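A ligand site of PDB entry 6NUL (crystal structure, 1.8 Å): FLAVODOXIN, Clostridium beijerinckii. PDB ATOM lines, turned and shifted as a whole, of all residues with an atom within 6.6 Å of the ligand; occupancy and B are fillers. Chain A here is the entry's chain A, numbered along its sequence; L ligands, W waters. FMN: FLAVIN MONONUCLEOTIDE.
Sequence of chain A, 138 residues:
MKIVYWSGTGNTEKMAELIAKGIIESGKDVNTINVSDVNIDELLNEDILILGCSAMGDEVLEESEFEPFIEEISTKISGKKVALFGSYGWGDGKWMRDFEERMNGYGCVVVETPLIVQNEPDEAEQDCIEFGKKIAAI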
ATOM      1  N   TRP A   6     -13.173  13.203 -28.485  1.00  0.00           N
ATOM      2  CA  TRP A   6     -12.164  14.252 -28.465  1.00  0.00           C
ATOM      3  C   TRP A   6     -11.108  13.775 -29.465  1.00  0.00           C
ATOM      4  O   TRP A   6     -10.743  12.593 -29.470  1.00  0.00           O
ATOM      5  CB  TRP A   6     -11.488  14.424 -27.100  1.00  0.00           C
ATOM      6  CG  TRP A   6     -10.509  15.582 -27.138  1.00  0.00           C
ATOM      7  CD1 TRP A   6     -10.804  16.903 -26.948  1.00  0.00           C
ATOM      8  CD2 TRP A   6      -9.113  15.538 -27.518  1.00  0.00           C
ATOM      9  NE1 TRP A   6      -9.705  17.680 -27.207  1.00  0.00           N
ATOM     10  CE2 TRP A   6      -8.650  16.870 -27.559  1.00  0.00           C
ATOM     11  CE3 TRP A   6      -8.216  14.502 -27.834  1.00  0.00           C
ATOM     12  CZ2 TRP A   6      -7.332  17.196 -27.896  1.00  0.00           C
ATOM     13  CZ3 TRP A   6      -6.901  14.823 -28.179  1.00  0.00           C
ATOM     14  CH2 TRP A   6      -6.473  16.168 -28.204  1.00  0.00           C
ATOM     15  N   SER A   7     -10.659  14.682 -30.329  1.00  0.00           N
ATOM     16  CA  SER A   7      -9.629  14.350 -31.311  1.00  0.00           C
ATOM     17  C   SER A   7      -8.719  15.552 -31.475  1.00  0.00           C
ATOM     18  O   SER A   7      -9.204  16.676 -31.686  1.00  0.00           O
ATOM     19  CB  SER A   7     -10.288  13.988 -32.637  1.00  0.00           C
ATOM     20  OG  SER A   7      -9.310  13.570 -33.573  1.00  0.00           O
ATOM     21  N   GLY A   8      -7.418  15.339 -31.373  1.00  0.00           N
ATOM     22  CA  GLY A   8      -6.470  16.442 -31.501  1.00  0.00           C
ATOM     23  C   GLY A   8      -5.946  16.713 -32.891  1.00  0.00           C
ATOM     24  O   GLY A   8      -5.487  17.827 -33.176  1.00  0.00           O
ATOM     25  N   THR A   9      -5.930  15.698 -33.751  1.00  0.00           N
ATOM     26  CA  THR A   9      -5.456  15.867 -35.122  1.00  0.00           C
ATOM     27  C   THR A   9      -6.474  15.325 -36.128  1.00  0.00           C
ATOM     28  O   THR A   9      -6.284  15.432 -37.338  1.00  0.00           O
ATOM     29  CB  THR A   9      -4.067  15.174 -35.343  1.00  0.00           C
ATOM     30  OG1 THR A   9      -4.221  13.763 -35.493  1.00  0.00           O
ATOM     31  CG2 THR A   9      -3.133  15.447 -34.154  1.00  0.00           C
ATOM     32  N   GLY A  10      -7.564  14.742 -35.624  1.00  0.00           N
ATOM     33  CA  GLY A  10      -8.593  14.223 -36.505  1.00  0.00           C
ATOM     34  C   GLY A  10      -8.673  12.715 -36.646  1.00  0.00           C
ATOM     35  O   GLY A  10      -9.587  12.216 -37.297  1.00  0.00           O
ATOM     36  N   ASN A  11      -7.756  11.984 -36.030  1.00  0.00           N
ATOM     37  CA  ASN A  11      -7.747  10.522 -36.145  1.00  0.00           C
ATOM     38  C   ASN A  11      -8.947   9.887 -35.460  1.00  0.00           C
ATOM     39  O   ASN A  11      -9.678   9.094 -36.078  1.00  0.00           O
ATOM     40  CB  ASN A  11      -6.426   9.932 -35.645  1.00  0.00           C
ATOM     41  CG  ASN A  11      -5.228  10.318 -36.530  1.00  0.00           C
ATOM     42  OD1 ASN A  11      -4.081  10.269 -36.085  1.00  0.00           O
ATOM     43  ND2 ASN A  11      -5.501  10.680 -37.776  1.00  0.00           N
ATOM     44  N   THR A  12      -9.208  10.276 -34.214  1.00  0.00           N
ATOM     45  CA  THR A  12     -10.371   9.771 -33.489  1.00  0.00           C
ATOM     46  C   THR A  12     -11.668  10.322 -34.082  1.00  0.00           C
ATOM     47  O   THR A  12     -12.690   9.642 -34.105  1.00  0.00           O
ATOM     48  CB  THR A  12     -10.268  10.057 -31.985  1.00  0.00           C
ATOM     49  OG1 THR A  12      -9.074   9.456 -31.484  1.00  0.00           O
ATOM     50  CG2 THR A  12     -11.451   9.444 -31.246  1.00  0.00           C
ATOM     51  N   GLU A  13     -11.611  11.531 -34.643  1.00  0.00           N
ATOM     52  CA  GLU A  13     -12.785  12.129 -35.296  1.00  0.00           C
ATOM     53  C   GLU A  13     -13.185  11.275 -36.516  1.00  0.00           C
ATOM     54  O   GLU A  13     -14.370  11.000 -36.747  1.00  0.00           O
ATOM     55  CB  GLU A  13     -12.470  13.553 -35.748  1.00  0.00           C
ATOM     56  CG  GLU A  13     -13.626  14.215 -36.484  1.00  0.00           C
ATOM     57  CD  GLU A  13     -13.287  15.615 -36.990  1.00  0.00           C
ATOM     58  OE1 GLU A  13     -12.105  15.908 -37.247  1.00  0.00           O
ATOM     59  OE2 GLU A  13     -14.224  16.427 -37.134  1.00  0.00           O
ATOM     60  N   CYS A  53     -11.720   8.823 -27.397  1.00  0.00           N
ATOM     61  CA  CYS A  53     -10.632   9.755 -27.124  1.00  0.00           C
ATOM     62  C   CYS A  53      -9.312   9.049 -27.411  1.00  0.00           C
ATOM     63  O   CYS A  53      -9.135   7.877 -27.076  1.00  0.00           O
ATOM     64  CB  CYS A  53     -10.646  10.207 -25.658  1.00  0.00           C
ATOM     65  SG  CYS A  53      -9.397  11.456 -25.245  1.00  0.00           S
ATOM     66  N   SER A  54      -8.399   9.768 -28.060  1.00  0.00           N
ATOM     67  CA  SER A  54      -7.079   9.233 -28.379  1.00  0.00           C
ATOM     68  C   SER A  54      -6.226   9.126 -27.123  1.00  0.00           C
ATOM     69  O   SER A  54      -6.586   9.668 -26.060  1.00  0.00           O
ATOM     70  CB  SER A  54      -6.394  10.150 -29.379  1.00  0.00           C
ATOM     71  OG  SER A  54      -6.512  11.496 -28.960  1.00  0.00           O
ATOM     72  N   ALA A  55      -5.118   8.390 -27.244  1.00  0.00           N
ATOM     73  CA  ALA A  55      -4.153   8.236 -26.157  1.00  0.00           C
ATOM     74  C   ALA A  55      -3.442   9.579 -26.021  1.00  0.00           C
ATOM     75  O   ALA A  55      -2.922  10.120 -27.014  1.00  0.00           O
ATOM     76  CB  ALA A  55      -3.150   7.131 -26.492  1.00  0.00           C
ATOM     77  N   MET A  56      -3.455  10.143 -24.822  1.00  0.00           N
ATOM     78  CA  MET A  56      -2.802  11.431 -24.557  1.00  0.00           C
ATOM     79  C   MET A  56      -1.875  11.331 -23.355  1.00  0.00           C
ATOM     80  O   MET A  56      -1.778  10.283 -22.728  1.00  0.00           O
ATOM     81  CB  MET A  56      -3.844  12.535 -24.356  1.00  0.00           C
ATOM     82  CG  MET A  56      -4.525  12.951 -25.666  1.00  0.00           C
ATOM     83  SD  MET A  56      -3.311  13.612 -26.862  1.00  0.00           S
ATOM     84  CE  MET A  56      -3.284  15.270 -26.330  1.00  0.00           C
ATOM     85  N   GLY A  57      -1.166  12.426 -23.065  1.00  0.00           N
ATOM     86  CA  GLY A  57      -0.230  12.455 -21.959  1.00  0.00           C
ATOM     87  C   GLY A  57       0.626  11.209 -21.996  1.00  0.00           C
ATOM     88  O   GLY A  57       1.240  10.884 -23.023  1.00  0.00           O
ATOM     89  N   ASP A  58       0.694  10.509 -20.874  1.00  0.00           N
ATOM     90  CA  ASP A  58       1.427   9.251 -20.837  1.00  0.00           C
ATOM     91  C   ASP A  58       0.345   8.209 -20.615  1.00  0.00           C
ATOM     92  O   ASP A  58      -0.011   7.901 -19.481  1.00  0.00           O
ATOM     93  CB  ASP A  58       2.444   9.228 -19.689  1.00  0.00           C
ATOM     94  CG  ASP A  58       3.299   7.974 -19.721  1.00  0.00           C
ATOM     95  OD1 ASP A  58       3.229   7.208 -20.706  1.00  0.00           O
ATOM     96  OD2 ASP A  58       4.059   7.746 -18.738  1.00  0.00           O
ATOM     97  N   GLU A  59      -0.253   7.771 -21.719  1.00  0.00           N
ATOM     98  CA  GLU A  59      -1.323   6.780 -21.693  1.00  0.00           C
ATOM     99  C   GLU A  59      -2.519   7.180 -20.830  1.00  0.00           C
ATOM    100  O   GLU A  59      -3.000   6.377 -20.032  1.00  0.00           O
ATOM    101  CB  GLU A  59      -0.776   5.418 -21.233  1.00  0.00           C
ATOM    102  CG  GLU A  59       0.291   4.816 -22.147  1.00  0.00           C
ATOM    103  CD  GLU A  59      -0.239   4.351 -23.503  1.00  0.00           C
ATOM    104  OE1 GLU A  59      -1.470   4.314 -23.705  1.00  0.00           O
ATOM    105  OE2 GLU A  59       0.587   4.036 -24.376  1.00  0.00           O
ATOM    106  N   VAL A  60      -3.016   8.395 -20.996  1.00  0.00           N
ATOM    107  CA  VAL A  60      -4.178   8.841 -20.223  1.00  0.00           C
ATOM    108  C   VAL A  60      -5.186   9.479 -21.178  1.00  0.00           C
ATOM    109  O   VAL A  60      -4.884   9.674 -22.347  1.00  0.00           O
ATOM    110  CB  VAL A  60      -3.792   9.897 -19.134  1.00  0.00           C
ATOM    111  CG1 VAL A  60      -2.828   9.289 -18.121  1.00  0.00           C
ATOM    112  CG2 VAL A  60      -3.182  11.143 -19.786  1.00  0.00           C
ATOM    113  N   GLY A  86     -10.853   4.792 -29.659  1.00  0.00           N
ATOM    114  CA  GLY A  86      -9.875   5.849 -29.744  1.00  0.00           C
ATOM    115  C   GLY A  86      -8.687   5.447 -30.591  1.00  0.00           C
ATOM    116  O   GLY A  86      -8.431   4.255 -30.810  1.00  0.00           O
ATOM    117  N   SER A  87      -7.971   6.454 -31.081  1.00  0.00           N
ATOM    118  CA  SER A  87      -6.774   6.252 -31.896  1.00  0.00           C
ATOM    119  C   SER A  87      -5.568   6.378 -30.954  1.00  0.00           C
ATOM    120  O   SER A  87      -5.644   7.062 -29.930  1.00  0.00           O
ATOM    121  CB  SER A  87      -6.708   7.335 -32.982  1.00  0.00           C
ATOM    122  OG  SER A  87      -5.571   7.169 -33.822  1.00  0.00           O
ATOM    123  N   TYR A  88      -4.471   5.704 -31.294  1.00  0.00           N
ATOM    124  CA  TYR A  88      -3.246   5.771 -30.495  1.00  0.00           C
ATOM    125  C   TYR A  88      -2.035   5.782 -31.421  1.00  0.00           C
ATOM    126  O   TYR A  88      -2.170   5.548 -32.627  1.00  0.00           O
ATOM    127  CB  TYR A  88      -3.157   4.638 -29.467  1.00  0.00           C
ATOM    128  CG  TYR A  88      -3.044   3.264 -30.076  1.00  0.00           C
ATOM    129  CD1 TYR A  88      -4.153   2.648 -30.637  1.00  0.00           C
ATOM    130  CD2 TYR A  88      -1.826   2.597 -30.095  1.00  0.00           C
ATOM    131  CE1 TYR A  88      -4.050   1.382 -31.211  1.00  0.00           C
ATOM    132  CE2 TYR A  88      -1.723   1.330 -30.669  1.00  0.00           C
ATOM    133  CZ  TYR A  88      -2.838   0.731 -31.225  1.00  0.00           C
ATOM    134  OH  TYR A  88      -2.743  -0.509 -31.813  1.00  0.00           O
ATOM    135  N   GLY A  89      -0.862   6.003 -30.834  1.00  0.00           N
ATOM    136  CA  GLY A  89       0.353   6.107 -31.636  1.00  0.00           C
ATOM    137  C   GLY A  89       1.415   5.066 -31.405  1.00  0.00           C
ATOM    138  O   GLY A  89       1.426   4.064 -32.099  1.00  0.00           O
ATOM    139  N   TRP A  90       2.260   5.259 -30.406  1.00  0.00           N
ATOM    140  CA  TRP A  90       3.371   4.344 -30.122  1.00  0.00           C
ATOM    141  C   TRP A  90       3.122   3.222 -29.121  1.00  0.00           C
ATOM    142  O   TRP A  90       3.915   2.280 -29.030  1.00  0.00           O
ATOM    143  CB  TRP A  90       4.598   5.149 -29.696  1.00  0.00           C
ATOM    144  CG  TRP A  90       4.313   6.095 -28.553  1.00  0.00           C
ATOM    145  CD1 TRP A  90       4.315   5.793 -27.214  1.00  0.00           C
ATOM    146  CD2 TRP A  90       3.973   7.485 -28.648  1.00  0.00           C
ATOM    147  NE1 TRP A  90       3.991   6.906 -26.482  1.00  0.00           N
ATOM    148  CE2 TRP A  90       3.786   7.960 -27.334  1.00  0.00           C
ATOM    149  CE3 TRP A  90       3.821   8.377 -29.725  1.00  0.00           C
ATOM    150  CZ2 TRP A  90       3.437   9.293 -27.059  1.00  0.00           C
ATOM    151  CZ3 TRP A  90       3.471   9.701 -29.445  1.00  0.00           C
ATOM    152  CH2 TRP A  90       3.286  10.139 -28.133  1.00  0.00           C
ATOM    153  N   GLY A  91       2.043   3.324 -28.334  1.00  0.00           N
ATOM    154  CA  GLY A  91       1.749   2.301 -27.353  1.00  0.00           C
ATOM    155  C   GLY A  91       1.013   1.103 -27.914  1.00  0.00           C
ATOM    156  O   GLY A  91       1.067   0.819 -29.118  1.00  0.00           O
ATOM    157  N   ASP A  92       0.325   0.374 -27.030  1.00  0.00           N
ATOM    158  CA  ASP A  92      -0.457  -0.780 -27.455  1.00  0.00           C
ATOM    159  C   ASP A  92      -1.836  -0.825 -26.805  1.00  0.00           C
ATOM    160  O   ASP A  92      -2.447  -1.883 -26.711  1.00  0.00           O
ATOM    161  CB  ASP A  92       0.308  -2.088 -27.214  1.00  0.00           C
ATOM    162  CG  ASP A  92       0.666  -2.315 -25.750  1.00  0.00           C
ATOM    163  OD1 ASP A  92       0.086  -1.676 -24.843  1.00  0.00           O
ATOM    164  OD2 ASP A  92       1.540  -3.176 -25.505  1.00  0.00           O
ATOM    165  N   GLY A  93      -2.307   0.316 -26.308  1.00  0.00           N
ATOM    166  CA  GLY A  93      -3.640   0.354 -25.726  1.00  0.00           C
ATOM    167  C   GLY A  93      -3.768   0.555 -24.237  1.00  0.00           C
ATOM    168  O   GLY A  93      -4.885   0.498 -23.719  1.00  0.00           O
ATOM    169  N   TRP A  95      -3.888   3.197 -22.340  1.00  0.00           N
ATOM    170  CA  TRP A  95      -4.875   4.210 -21.978  1.00  0.00           C
ATOM    171  C   TRP A  95      -6.303   3.679 -22.102  1.00  0.00           C
ATOM    172  O   TRP A  95      -7.172   4.049 -21.296  1.00  0.00           O
ATOM    173  CB  TRP A  95      -4.679   5.496 -22.806  1.00  0.00           C
ATOM    174  CG  TRP A  95      -5.666   5.706 -23.958  1.00  0.00           C
ATOM    175  CD1 TRP A  95      -6.686   6.616 -23.999  1.00  0.00           C
ATOM    176  CD2 TRP A  95      -5.707   4.986 -25.201  1.00  0.00           C
ATOM    177  NE1 TRP A  95      -7.368   6.503 -25.202  1.00  0.00           N
ATOM    178  CE2 TRP A  95      -6.791   5.512 -25.951  1.00  0.00           C
ATOM    179  CE3 TRP A  95      -4.941   3.959 -25.760  1.00  0.00           C
ATOM    180  CZ2 TRP A  95      -7.117   5.045 -27.229  1.00  0.00           C
ATOM    181  CZ3 TRP A  95      -5.271   3.479 -27.040  1.00  0.00           C
ATOM    182  CH2 TRP A  95      -6.344   4.026 -27.758  1.00  0.00           C
ATOM    183  N   VAL A 117      -7.390   1.969 -32.828  1.00  0.00           N
ATOM    184  CA  VAL A 117      -6.767   2.006 -34.144  1.00  0.00           C
ATOM    185  C   VAL A 117      -5.541   2.888 -34.059  1.00  0.00           C
ATOM    186  O   VAL A 117      -5.551   3.927 -33.400  1.00  0.00           O
ATOM    187  CB  VAL A 117      -7.769   2.563 -35.186  1.00  0.00           C
ATOM    188  CG1 VAL A 117      -7.081   2.860 -36.515  1.00  0.00           C
ATOM    189  CG2 VAL A 117      -8.883   1.559 -35.407  1.00  0.00           C
ATOM    190  N   GLN A 118      -4.464   2.452 -34.699  1.00  0.00           N
ATOM    191  CA  GLN A 118      -3.226   3.209 -34.675  1.00  0.00           C
ATOM    192  C   GLN A 118      -3.231   4.318 -35.729  1.00  0.00           C
ATOM    193  O   GLN A 118      -3.460   4.060 -36.912  1.00  0.00           O
ATOM    194  CB  GLN A 118      -2.038   2.262 -34.890  1.00  0.00           C
ATOM    195  CG  GLN A 118      -0.700   2.893 -34.552  1.00  0.00           C
ATOM    196  CD  GLN A 118       0.469   1.964 -34.832  1.00  0.00           C
ATOM    197  OE1 GLN A 118       0.299   0.732 -34.892  1.00  0.00           O
ATOM    198  NE2 GLN A 118       1.666   2.541 -34.964  1.00  0.00           N
ATOM    199  N   ASN A 119      -3.030   5.549 -35.262  1.00  0.00           N
ATOM    200  CA  ASN A 119      -2.985   6.738 -36.112  1.00  0.00           C
ATOM    201  C   ASN A 119      -4.279   6.868 -36.949  1.00  0.00           C
ATOM    202  O   ASN A 119      -5.355   6.543 -36.450  1.00  0.00           O
ATOM    203  CB  ASN A 119      -1.730   6.711 -36.981  1.00  0.00           C
ATOM    204  CG  ASN A 119      -0.465   6.457 -36.156  1.00  0.00           C
ATOM    205  OD1 ASN A 119      -0.161   7.165 -35.191  1.00  0.00           O
ATOM    206  ND2 ASN A 119       0.267   5.429 -36.519  1.00  0.00           N
ATOM    207  N   GLU A 120      -4.214   7.377 -38.181  1.00  0.00           N
ATOM    208  CA  GLU A 120      -5.449   7.488 -38.965  1.00  0.00           C
ATOM    209  C   GLU A 120      -5.876   6.091 -39.387  1.00  0.00           C
ATOM    210  O   GLU A 120      -5.042   5.285 -39.799  1.00  0.00           O
ATOM    211  CB  GLU A 120      -5.272   8.373 -40.212  1.00  0.00           C
ATOM    212  CG  GLU A 120      -6.627   8.746 -40.847  1.00  0.00           C
ATOM    213  CD  GLU A 120      -6.526   9.503 -42.172  1.00  0.00           C
ATOM    214  OE1 GLU A 120      -5.866  10.570 -42.191  1.00  0.00           O
ATOM    215  OE2 GLU A 120      -7.109   9.041 -43.181  1.00  0.00           O
HETATM  216  N1  FMN L   1      -0.040   7.334 -28.289  1.00  0.00           N
HETATM  217  C2  FMN L   1       0.112   6.190 -27.546  1.00  0.00           C
HETATM  218  O2  FMN L   1       0.001   5.078 -28.057  1.00  0.00           O
HETATM  219  N3  FMN L   1       0.387   6.330 -26.171  1.00  0.00           N
HETATM  220  C4  FMN L   1       0.431   7.533 -25.473  1.00  0.00           C
HETATM  221  O4  FMN L   1       0.680   7.583 -24.278  1.00  0.00           O
HETATM  222  C4A FMN L   1       0.226   8.763 -26.312  1.00  0.00           C
HETATM  223  N5  FMN L   1       0.325   9.974 -25.760  1.00  0.00           N
HETATM  224  C5A FMN L   1       0.292  11.083 -26.596  1.00  0.00           C
HETATM  225  C6  FMN L   1       0.569  12.374 -26.082  1.00  0.00           C
HETATM  226  C7  FMN L   1       0.567  13.505 -26.844  1.00  0.00           C
HETATM  227  C7M FMN L   1       0.956  14.816 -26.209  1.00  0.00           C
HETATM  228  C8  FMN L   1       0.198  13.403 -28.210  1.00  0.00           C
HETATM  229  C8M FMN L   1      -0.038  14.611 -29.123  1.00  0.00           C
HETATM  230  C9  FMN L   1      -0.016  12.138 -28.750  1.00  0.00           C
HETATM  231  C9A FMN L   1       0.015  10.972 -27.964  1.00  0.00           C
HETATM  232  N10 FMN L   1      -0.142   9.678 -28.505  1.00  0.00           N
HETATM  233  C10 FMN L   1      -0.021   8.540 -27.719  1.00  0.00           C
HETATM  234  C1' FMN L   1      -0.395   9.532 -29.922  1.00  0.00           C
HETATM  235  C2' FMN L   1      -1.853   9.795 -30.281  1.00  0.00           C
HETATM  236  O2' FMN L   1      -2.711   8.984 -29.471  1.00  0.00           O
HETATM  237  C3' FMN L   1      -2.084   9.469 -31.753  1.00  0.00           C
HETATM  238  O3' FMN L   1      -1.291  10.328 -32.571  1.00  0.00           O
HETATM  239  C4' FMN L   1      -3.531   9.479 -32.241  1.00  0.00           C
HETATM  240  O4' FMN L   1      -3.578   9.030 -33.602  1.00  0.00           O
HETATM  241  C5' FMN L   1      -4.137  10.885 -32.071  1.00  0.00           C
HETATM  242  O5' FMN L   1      -5.519  10.864 -32.416  1.00  0.00           O
HETATM  243  P   FMN L   1      -6.313  12.178 -32.504  1.00  0.00           P
HETATM  244  O1P FMN L   1      -5.954  12.878 -33.735  1.00  0.00           O
HETATM  245  O2P FMN L   1      -7.703  11.758 -32.414  1.00  0.00           O
HETATM  246  O3P FMN L   1      -5.906  12.997 -31.263  1.00  0.00           O
HETATM  247  O   HOH W   1      -3.554  13.925 -30.332  1.00  0.00           O
HETATM  248  O   HOH W   2      -1.637   3.125 -26.368  1.00  0.00           O
HETATM  249  O   HOH W   3      -1.514  13.050 -32.109  1.00  0.00           O
HETATM  250  O   HOH W   4       3.268   7.406 -23.600  1.00  0.00           O
HETATM  251  O   HOH W   5      -0.787   9.752 -35.121  1.00  0.00           O
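An oxygen (O4) of the ligand is in hydrogen-bond range of the backbone NH of Glu 59, at 2.7 Å. OG of Ser 54 is in hydrogen-bond range of O3P of the ligand, 2.8 Å away. The backbone NH (N) of Ala 55 is in hydrogen-bond range of an oxygen (O2') of the ligand. The side-chain hydroxyl (OG) of Ser 7 sits at hydrogen-bond distance from an oxygen (O2P) of the ligand, 2.7 Å away. N of Thr 9 lies within hydrogen-bond range of O1P of the ligand (2.8 Å). The backbone NH of Gly 8 sits at hydrogen-bond distance from an oxygen (O3P) of the ligand, at 2.8 Å. N1 of the ligand lies within hydrogen-bond range of N of Gly 89 (3.0 Å). OG1 of Thr 12 lies within hydrogen-bond range of O2P of the ligand, 2.8 Å away. The side-chain hydroxyl (OG) of Ser 87 is in hydrogen-bond range of an oxygen (O4') of the ligand, 2.7 Å away. OD1 of Asn 11 is in hydrogen-bond range of O4' of the ligand, 2.8 Å away. OG1 of Thr 9 sits at hydrogen-bond distance from O1P of the ligand, 2.6 Å away. OE2 of Glu 59 lies within hydrogen-bond range of N3 of the ligand, at 2.9 Å. The backbone carbonyl oxygen of Ala 55 sits at hydrogen-bond distance from an oxygen (O2') of the ligand (2.7 Å). The backbone NH (N) of Thr 12 sits at hydrogen-bond distance from an oxygen (O2P) of the ligand (2.8 Å). The backbone NH of Trp 90 is in hydrogen-bond range of an oxygen (O2) of the ligand (3.3 Å). The backbone NH (N) of Gly 10 sits at hydrogen-bond distance from an oxygen (O1P) of the ligand (3.1 Å). O1P of the ligand sits at hydrogen-bond distance from N of Asn 11, 3.1 Å away. N of Gly 91 sits at hydrogen-bond distance from O2 of the ligand, at 2.7 Å.
OG of Ser 87 is in hydrogen-bond range of O of Asn 119 (2.7 Å). The backbone NH of Trp 95 is in hydrogen-bond range of the side-chain carboxylate of Glu 59, 3.0 Å away. O of Ser 54 lies within hydrogen-bond range of NE1 of Trp 95 (3.4 Å). O of Tyr 88 is in hydrogen-bond range of N of Asn 119 (2.8 Å). OG of Ser 7 lies within hydrogen-bond range of N of Asn 11, at 3.3 Å. N of Ser 87 lies within hydrogen-bond range of OG1 of Thr 12, at 3.2 Å. O of Val 117 lies close to OG of Ser 87 (3.3 Å). The backbone carbonyl oxygen of Ser 87 sits at hydrogen-bond distance from the backbone NH of Ala 55, 3.0 Å away.
The backbone carbonyl oxygen of Gly 57 sits close to a nitrogen (N5) of the ligand (3.0 Å). Trp 6 touches the ligand. Met 56 touches the ligand (C to N5, 3.5 Å). C of Asp 58 touches O4 of the ligand, 3.7 Å away. CA of Tyr 88 touches O2' of the ligand, at 3.4 Å. Asn 119 touches the ligand. Hydrophobic or aromatic side chains within 4 Å of the ligand: Trp 6, Ala 55, Met 56, Tyr 88 and Trp 90. Within 4 Å of the ligand: Trp 6, Ser 7, Gly 8, Thr 9, Gly 10, Asn 11, Thr 12, Ser 54, Ala 55, Met 56, Gly 57, Asp 58, Glu 59, Ser 87, Tyr 88, Gly 89, Trp 90, Gly 91 and Asn 119.
Water W5 lies within hydrogen-bond range of OD1 of Asn 119 (2.7 Å), O3' of the ligand (2.7 Å) and OD1 of Asn 11 (3.5 Å). Water W4 lies within hydrogen-bond range of O4 of the ligand (2.7 Å), OD1 of Asp 58 (2.9 Å) and NE1 of Trp 90 (3.0 Å). Water W1 lies within hydrogen-bond range of O3P of the ligand (2.7 Å) and SD of Met 56 (3.5 Å). Water W2 lies within hydrogen-bond range of N of Gly 93 (2.9 Å), OE1 of Glu 59 (2.9 Å), O2 of the ligand (3.1 Å) and N of Asp 92 (3.4 Å).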
